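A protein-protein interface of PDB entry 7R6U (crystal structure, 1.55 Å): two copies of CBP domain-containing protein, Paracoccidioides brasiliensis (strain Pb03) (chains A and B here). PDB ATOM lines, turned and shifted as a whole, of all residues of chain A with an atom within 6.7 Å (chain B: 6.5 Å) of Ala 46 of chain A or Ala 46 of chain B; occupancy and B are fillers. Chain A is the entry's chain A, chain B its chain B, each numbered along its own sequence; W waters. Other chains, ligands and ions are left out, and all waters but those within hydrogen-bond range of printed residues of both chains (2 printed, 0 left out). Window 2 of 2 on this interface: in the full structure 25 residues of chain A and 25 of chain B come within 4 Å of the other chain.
Of the 15 printed residues of chain A, 4 touch a printed residue of chain B. Printed residues of chain A that touch a printed residue of chain B: Ala 42, Ala 46, Glu 50 and Leu 57. Along chain A the printed residues that touch a printed residue of chain B span positions 42 to 57. Of the 15 printed residues of chain B, 5 touch a printed residue of chain A. Hydrophobic or aromatic side chains of chain B within 4 Å of the printed part of chain A: Ala 42, Ala 43, Ala 46 and Leu 57. Along chain B the printed residues that touch a printed residue of chain A span positions 42 to 57. Among the printed residues, 5 pairs touch across the chains. Among the printed residues, no Asp or Glu carboxylate lies within 4 Å of a Lys or Arg side-chain nitrogen of the other chain.
N of Leu 57 of chain A sits at hydrogen-bond distance from OD1 of Asp 54 of chain A, 3.2 Å away. N of Ala 43 of chain B sits close to OG of Ser 41 of chain B (3.4 Å). N of Leu 57 of chain B is in hydrogen-bond range of OD1 of Asp 54 of chain B, 3.2 Å away.
Among the printed residues, pairs that only touch across the chains: Ala 42 of chain A with Glu 50 of chain B (3.3 Å), Glu 50 of chain A with Ala 42 of chain B (3.5 Å), Leu 57 of chain A with Leu 57 of chain B (3.6 Å), Ala 46 of chain A with Ala 46 of chain B (3.7 Å) and Leu 57 of chain A with Ala 43 of chain B (3.99 Å).
Of chain A, only Ala 46 comes within 4 Å of Ala 46 of chain B. Of the printed residues of chain A, Ala 42 of chain B touches Glu 50. Printed residues of chain B within 4 Å of Glu 50 of chain A: Ala 42. Printed residues of chain A within 4 Å of Glu 50 of chain B: Ala 42. Of the printed residues of chain B, Ala 42 of chain A touches Glu 50. Asp 54 of chain B touches none of the printed residues of chain A. Ser 41 of chain A touches none of the printed residues of chain B. The nearest residue of chain B that does not touch Ala 46 of chain A is Ala 42 of chain B (5.1 Å).
Ala 42 of chain A touches Glu 50 of chain B, and with the chains exchanged Glu 50 of chain A touches Ala 42 of chain B. Ala 46 of chain B touches its own counterpart, Ala 46 of chain A. Leu 57 of chain A touches Ala 43 of chain B, but with the chains exchanged Ala 43 of chain A does not touch Leu 57 of chain B (4.1 Å). Leu 57 of chain B touches its own counterpart, Leu 57 of chain A.
Water W2 lies within hydrogen-bond range of the side-chain carboxylate (OD2) of Asp 54 of chain B (2.7 Å) and the backbone NH (N) of Ala 43 of chain A (3.0 Å). Water W1 lies within hydrogen-bond range of the side-chain carboxylate of Asp 54 of chain A and the backbone NH of Ala 43 of chain B.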
ATOM      1  N   ALA A  38      -3.244  -1.352  26.289  1.00  0.00           N
ATOM      2  CA  ALA A  38      -2.434  -2.445  25.745  1.00  0.00           C
ATOM      3  C   ALA A  38      -3.052  -3.059  24.490  1.00  0.00           C
ATOM      4  O   ALA A  38      -2.329  -3.531  23.607  1.00  0.00           O
ATOM      5  CB  ALA A  38      -2.224  -3.524  26.803  1.00  0.00           C
ATOM      6  N   SER A  41      -2.319  -0.855  20.547  1.00  0.00           N
ATOM      7  CA  SER A  41      -1.189  -0.738  19.631  1.00  0.00           C
ATOM      8  C   SER A  41      -0.096  -1.708  20.040  1.00  0.00           C
ATOM      9  O   SER A  41      -0.016  -2.141  21.192  1.00  0.00           O
ATOM     10  CB  SER A  41      -0.618   0.687  19.586  1.00  0.00           C
ATOM     11  OG  SER A  41       0.303   0.922  20.652  1.00  0.00           O
ATOM     12  N   ALA A  42       0.767  -2.020  19.069  1.00  0.00           N
ATOM     13  CA  ALA A  42       1.888  -2.911  19.331  1.00  0.00           C
ATOM     14  C   ALA A  42       2.828  -2.315  20.362  1.00  0.00           C
ATOM     15  O   ALA A  42       3.361  -3.036  21.213  1.00  0.00           O
ATOM     16  CB  ALA A  42       2.642  -3.199  18.036  1.00  0.00           C
ATOM     17  N   ALA A  43       3.047  -1.002  20.299  1.00  0.00           N
ATOM     18  CA  ALA A  43       3.942  -0.353  21.248  1.00  0.00           C
ATOM     19  C   ALA A  43       3.401  -0.459  22.665  1.00  0.00           C
ATOM     20  O   ALA A  43       4.163  -0.668  23.616  1.00  0.00           O
ATOM     21  CB  ALA A  43       4.145   1.112  20.865  1.00  0.00           C
ATOM     22  N   CYS A  44       2.086  -0.302  22.827  1.00  0.00           N
ATOM     23  CA  CYS A  44       1.504  -0.338  24.166  1.00  0.00           C
ATOM     24  C   CYS A  44       1.542  -1.742  24.761  1.00  0.00           C
ATOM     25  O   CYS A  44       1.803  -1.912  25.960  1.00  0.00           O
ATOM     26  CB  CYS A  44       0.077   0.208  24.114  1.00  0.00           C
ATOM     27  SG  CYS A  44       0.082   2.009  23.715  1.00  0.00           S
ATOM     28  N   ALA A  45       1.274  -2.764  23.950  1.00  0.00           N
ATOM     29  CA  ALA A  45       1.394  -4.128  24.447  1.00  0.00           C
ATOM     30  C   ALA A  45       2.826  -4.428  24.876  1.00  0.00           C
ATOM     31  O   ALA A  45       3.055  -5.075  25.905  1.00  0.00           O
ATOM     32  CB  ALA A  45       0.932  -5.101  23.374  1.00  0.00           C
ATOM     33  N   ALA A  46       3.804  -3.959  24.100  1.00  0.00           N
ATOM     34  CA  ALA A  46       5.204  -4.152  24.471  1.00  0.00           C
ATOM     35  C   ALA A  46       5.557  -3.387  25.745  1.00  0.00           C
ATOM     36  O   ALA A  46       6.265  -3.914  26.612  1.00  0.00           O
ATOM     37  CB  ALA A  46       6.107  -3.711  23.322  1.00  0.00           C
ATOM     38  N   ALA A  47       5.080  -2.148  25.874  1.00  0.00           N
ATOM     39  CA  ALA A  47       5.360  -1.369  27.075  1.00  0.00           C
ATOM     40  C   ALA A  47       4.783  -2.038  28.320  1.00  0.00           C
ATOM     41  O   ALA A  47       5.420  -2.043  29.385  1.00  0.00           O
ATOM     42  CB  ALA A  47       4.806   0.048  26.921  1.00  0.00           C
ATOM     43  N   LEU A  48       3.578  -2.608  28.208  1.00  0.00           N
ATOM     44  CA  LEU A  48       2.981  -3.300  29.344  1.00  0.00           C
ATOM     45  C   LEU A  48       3.759  -4.562  29.690  1.00  0.00           C
ATOM     46  O   LEU A  48       3.892  -4.914  30.865  1.00  0.00           O
ATOM     47  CB  LEU A  48       1.517  -3.626  29.046  1.00  0.00           C
ATOM     48  CG  LEU A  48       0.803  -4.337  30.200  1.00  0.00           C
ATOM     49  CD1 LEU A  48       0.823  -3.507  31.476  1.00  0.00           C
ATOM     50  CD2 LEU A  48      -0.624  -4.678  29.804  1.00  0.00           C
ATOM     51  N   GLY A  49       4.296  -5.246  28.681  1.00  0.00           N
ATOM     52  CA  GLY A  49       5.094  -6.427  28.950  1.00  0.00           C
ATOM     53  C   GLY A  49       6.330  -6.124  29.772  1.00  0.00           C
ATOM     54  O   GLY A  49       6.825  -6.991  30.497  1.00  0.00           O
ATOM     55  N   GLU A  50       6.830  -4.886  29.693  1.00  0.00           N
ATOM     56  CA  GLU A  50       7.941  -4.423  30.508  1.00  0.00           C
ATOM     57  C   GLU A  50       7.474  -3.697  31.771  1.00  0.00           C
ATOM     58  O   GLU A  50       8.300  -3.084  32.464  1.00  0.00           O
ATOM     59  CB  GLU A  50       8.856  -3.517  29.668  1.00  0.00           C
ATOM     60  CG  GLU A  50       9.476  -4.249  28.477  1.00  0.00           C
ATOM     61  CD  GLU A  50      10.271  -5.469  28.910  1.00  0.00           C
ATOM     62  OE1 GLU A  50      11.281  -5.288  29.620  1.00  0.00           O
ATOM     63  OE2 GLU A  50       9.883  -6.606  28.562  1.00  0.00           O
ATOM     64  N   LEU A  51       6.172  -3.775  32.088  1.00  0.00           N
ATOM     65  CA  LEU A  51       5.609  -3.257  33.340  1.00  0.00           C
ATOM     66  C   LEU A  51       5.806  -1.749  33.482  1.00  0.00           C
ATOM     67  O   LEU A  51       5.846  -1.211  34.593  1.00  0.00           O
ATOM     68  CB  LEU A  51       6.159  -4.012  34.559  1.00  0.00           C
ATOM     69  CG  LEU A  51       5.940  -5.516  34.500  1.00  0.00           C
ATOM     70  CD1 LEU A  51       6.592  -6.213  35.672  1.00  0.00           C
ATOM     71  CD2 LEU A  51       4.448  -5.813  34.470  1.00  0.00           C
ATOM     72  N   GLY A  52       5.893  -1.051  32.353  1.00  0.00           N
ATOM     73  CA  GLY A  52       6.092   0.385  32.341  1.00  0.00           C
ATOM     74  C   GLY A  52       7.496   0.855  32.649  1.00  0.00           C
ATOM     75  O   GLY A  52       7.742   2.062  32.627  1.00  0.00           O
ATOM     76  N   ASP A  54      10.182   0.526  30.878  1.00  0.00           N
ATOM     77  CA  ASP A  54      10.943   0.824  29.663  1.00  0.00           C
ATOM     78  C   ASP A  54      10.419   2.153  29.126  1.00  0.00           C
ATOM     79  O   ASP A  54       9.404   2.195  28.431  1.00  0.00           O
ATOM     80  CB  ASP A  54      10.785  -0.330  28.672  1.00  0.00           C
ATOM     81  CG  ASP A  54      11.751  -0.259  27.492  1.00  0.00           C
ATOM     82  OD1 ASP A  54      11.897   0.817  26.877  1.00  0.00           O
ATOM     83  OD2 ASP A  54      12.343  -1.313  27.155  1.00  0.00           O
ATOM     84  N   LEU A  57       9.668   2.552  25.357  1.00  0.00           N
ATOM     85  CA  LEU A  57       8.430   1.906  24.943  1.00  0.00           C
ATOM     86  C   LEU A  57       7.208   2.652  25.476  1.00  0.00           C
ATOM     87  O   LEU A  57       6.192   2.732  24.777  1.00  0.00           O
ATOM     88  CB  LEU A  57       8.414   0.442  25.384  1.00  0.00           C
ATOM     89  CG  LEU A  57       9.398  -0.473  24.648  1.00  0.00           C
ATOM     90  CD1 LEU A  57       9.326  -1.892  25.213  1.00  0.00           C
ATOM     91  CD2 LEU A  57       9.123  -0.487  23.153  1.00  0.00           C
ATOM     92  N   ALA B  38      16.787  -8.862  17.364  1.00  0.00           N
ATOM     93  CA  ALA B  38      15.527  -9.119  18.055  1.00  0.00           C
ATOM     94  C   ALA B  38      15.730  -9.768  19.421  1.00  0.00           C
ATOM     95  O   ALA B  38      14.971  -9.485  20.355  1.00  0.00           O
ATOM     96  CB  ALA B  38      14.623  -9.986  17.189  1.00  0.00           C
ATOM     97  N   SER B  41      16.698  -7.140  22.999  1.00  0.00           N
ATOM     98  CA  SER B  41      15.917  -6.248  23.850  1.00  0.00           C
ATOM     99  C   SER B  41      14.433  -6.384  23.539  1.00  0.00           C
ATOM    100  O   SER B  41      14.035  -6.848  22.464  1.00  0.00           O
ATOM    101  CB  SER B  41      16.350  -4.786  23.690  1.00  0.00           C
ATOM    102  OG  SER B  41      15.729  -4.193  22.557  1.00  0.00           O
ATOM    103  N   ALA B  42      13.620  -5.959  24.509  1.00  0.00           N
ATOM    104  CA  ALA B  42      12.171  -5.970  24.342  1.00  0.00           C
ATOM    105  C   ALA B  42      11.739  -5.072  23.190  1.00  0.00           C
ATOM    106  O   ALA B  42      10.798  -5.402  22.456  1.00  0.00           O
ATOM    107  CB  ALA B  42      11.503  -5.522  25.641  1.00  0.00           C
ATOM    108  N   ALA B  43      12.395  -3.917  23.038  1.00  0.00           N
ATOM    109  CA  ALA B  43      12.052  -3.012  21.945  1.00  0.00           C
ATOM    110  C   ALA B  43      12.375  -3.638  20.598  1.00  0.00           C
ATOM    111  O   ALA B  43      11.596  -3.513  19.648  1.00  0.00           O
ATOM    112  CB  ALA B  43      12.777  -1.678  22.093  1.00  0.00           C
ATOM    113  N   CYS B  44      13.517  -4.327  20.496  1.00  0.00           N
ATOM    114  CA  CYS B  44      13.884  -4.907  19.207  1.00  0.00           C
ATOM    115  C   CYS B  44      12.959  -6.059  18.848  1.00  0.00           C
ATOM    116  O   CYS B  44      12.561  -6.206  17.683  1.00  0.00           O
ATOM    117  CB  CYS B  44      15.345  -5.356  19.219  1.00  0.00           C
ATOM    118  SG  CYS B  44      16.482  -3.921  19.315  1.00  0.00           S
ATOM    119  N   ALA B  45      12.584  -6.874  19.835  1.00  0.00           N
ATOM    120  CA  ALA B  45      11.625  -7.942  19.572  1.00  0.00           C
ATOM    121  C   ALA B  45      10.283  -7.381  19.109  1.00  0.00           C
ATOM    122  O   ALA B  45       9.683  -7.904  18.159  1.00  0.00           O
ATOM    123  CB  ALA B  45      11.447  -8.812  20.817  1.00  0.00           C
ATOM    124  N   ALA B  46       9.817  -6.293  19.742  1.00  0.00           N
ATOM    125  CA  ALA B  46       8.550  -5.685  19.335  1.00  0.00           C
ATOM    126  C   ALA B  46       8.651  -5.097  17.933  1.00  0.00           C
ATOM    127  O   ALA B  46       7.720  -5.220  17.128  1.00  0.00           O
ATOM    128  CB  ALA B  46       8.123  -4.608  20.334  1.00  0.00           C
ATOM    129  N   ALA B  47       9.776  -4.455  17.628  1.00  0.00           N
ATOM    130  CA  ALA B  47       9.948  -3.858  16.308  1.00  0.00           C
ATOM    131  C   ALA B  47       9.940  -4.916  15.211  1.00  0.00           C
ATOM    132  O   ALA B  47       9.353  -4.708  14.140  1.00  0.00           O
ATOM    133  CB  ALA B  47      11.247  -3.058  16.279  1.00  0.00           C
ATOM    134  N   LEU B  48      10.580  -6.066  15.456  1.00  0.00           N
ATOM    135  CA  LEU B  48      10.559  -7.131  14.459  1.00  0.00           C
ATOM    136  C   LEU B  48       9.152  -7.695  14.287  1.00  0.00           C
ATOM    137  O   LEU B  48       8.749  -8.036  13.170  1.00  0.00           O
ATOM    138  CB  LEU B  48      11.528  -8.250  14.848  1.00  0.00           C
ATOM    139  CG  LEU B  48      11.632  -9.424  13.871  1.00  0.00           C
ATOM    140  CD1 LEU B  48      12.134  -8.993  12.499  1.00  0.00           C
ATOM    141  CD2 LEU B  48      12.484 -10.522  14.455  1.00  0.00           C
ATOM    142  N   GLY B  49       8.385  -7.788  15.377  1.00  0.00           N
ATOM    143  CA  GLY B  49       7.013  -8.266  15.280  1.00  0.00           C
ATOM    144  C   GLY B  49       6.126  -7.394  14.415  1.00  0.00           C
ATOM    145  O   GLY B  49       5.136  -7.882  13.855  1.00  0.00           O
ATOM    146  N   GLU B  50       6.459  -6.110  14.294  1.00  0.00           N
ATOM    147  CA  GLU B  50       5.767  -5.186  13.409  1.00  0.00           C
ATOM    148  C   GLU B  50       6.451  -5.054  12.049  1.00  0.00           C
ATOM    149  O   GLU B  50       6.151  -4.119  11.304  1.00  0.00           O
ATOM    150  CB  GLU B  50       5.635  -3.817  14.073  1.00  0.00           C
ATOM    151  CG  GLU B  50       4.828  -3.883  15.353  1.00  0.00           C
ATOM    152  CD  GLU B  50       3.486  -4.551  15.134  1.00  0.00           C
ATOM    153  OE1 GLU B  50       2.666  -4.011  14.369  1.00  0.00           O
ATOM    154  OE2 GLU B  50       3.251  -5.629  15.730  1.00  0.00           O
ATOM    155  N   LEU B  51       7.372  -5.961  11.727  1.00  0.00           N
ATOM    156  CA  LEU B  51       8.014  -6.061  10.419  1.00  0.00           C
ATOM    157  C   LEU B  51       8.836  -4.827  10.075  1.00  0.00           C
ATOM    158  O   LEU B  51       9.083  -4.558   8.893  1.00  0.00           O
ATOM    159  CB  LEU B  51       6.976  -6.318   9.310  1.00  0.00           C
ATOM    160  CG  LEU B  51       6.017  -7.483   9.533  1.00  0.00           C
ATOM    161  CD1 LEU B  51       4.986  -7.490   8.437  1.00  0.00           C
ATOM    162  CD2 LEU B  51       6.738  -8.838   9.572  1.00  0.00           C
ATOM    163  N   GLY B  52       9.298  -4.091  11.085  1.00  0.00           N
ATOM    164  CA  GLY B  52      10.047  -2.872  10.852  1.00  0.00           C
ATOM    165  C   GLY B  52       9.216  -1.698  10.398  1.00  0.00           C
ATOM    166  O   GLY B  52       9.769  -0.614  10.170  1.00  0.00           O
ATOM    167  N   ASP B  54       6.991   0.018  12.052  1.00  0.00           N
ATOM    168  CA  ASP B  54       6.659   0.928  13.153  1.00  0.00           C
ATOM    169  C   ASP B  54       7.929   1.708  13.492  1.00  0.00           C
ATOM    170  O   ASP B  54       8.797   1.206  14.209  1.00  0.00           O
ATOM    171  CB  ASP B  54       6.143   0.094  14.325  1.00  0.00           C
ATOM    172  CG  ASP B  54       5.536   0.922  15.444  1.00  0.00           C
ATOM    173  OD1 ASP B  54       6.152   1.918  15.867  1.00  0.00           O
ATOM    174  OD2 ASP B  54       4.434   0.552  15.915  1.00  0.00           O
ATOM    175  N   LEU B  57       9.069   2.107  17.164  1.00  0.00           N
ATOM    176  CA  LEU B  57       9.680   0.909  17.737  1.00  0.00           C
ATOM    177  C   LEU B  57      11.065   0.655  17.154  1.00  0.00           C
ATOM    178  O   LEU B  57      11.960   0.199  17.873  1.00  0.00           O
ATOM    179  CB  LEU B  57       8.785  -0.312  17.515  1.00  0.00           C
ATOM    180  CG  LEU B  57       7.489  -0.348  18.333  1.00  0.00           C
ATOM    181  CD1 LEU B  57       6.687  -1.588  17.938  1.00  0.00           C
ATOM    182  CD2 LEU B  57       7.797  -0.354  19.834  1.00  0.00           C
HETATM  183  O   HOH W   1      14.036  -2.339  25.043  1.00  0.00           O
HETATM  184  O   HOH W   2       2.633   0.783  17.889  1.00  0.00           O
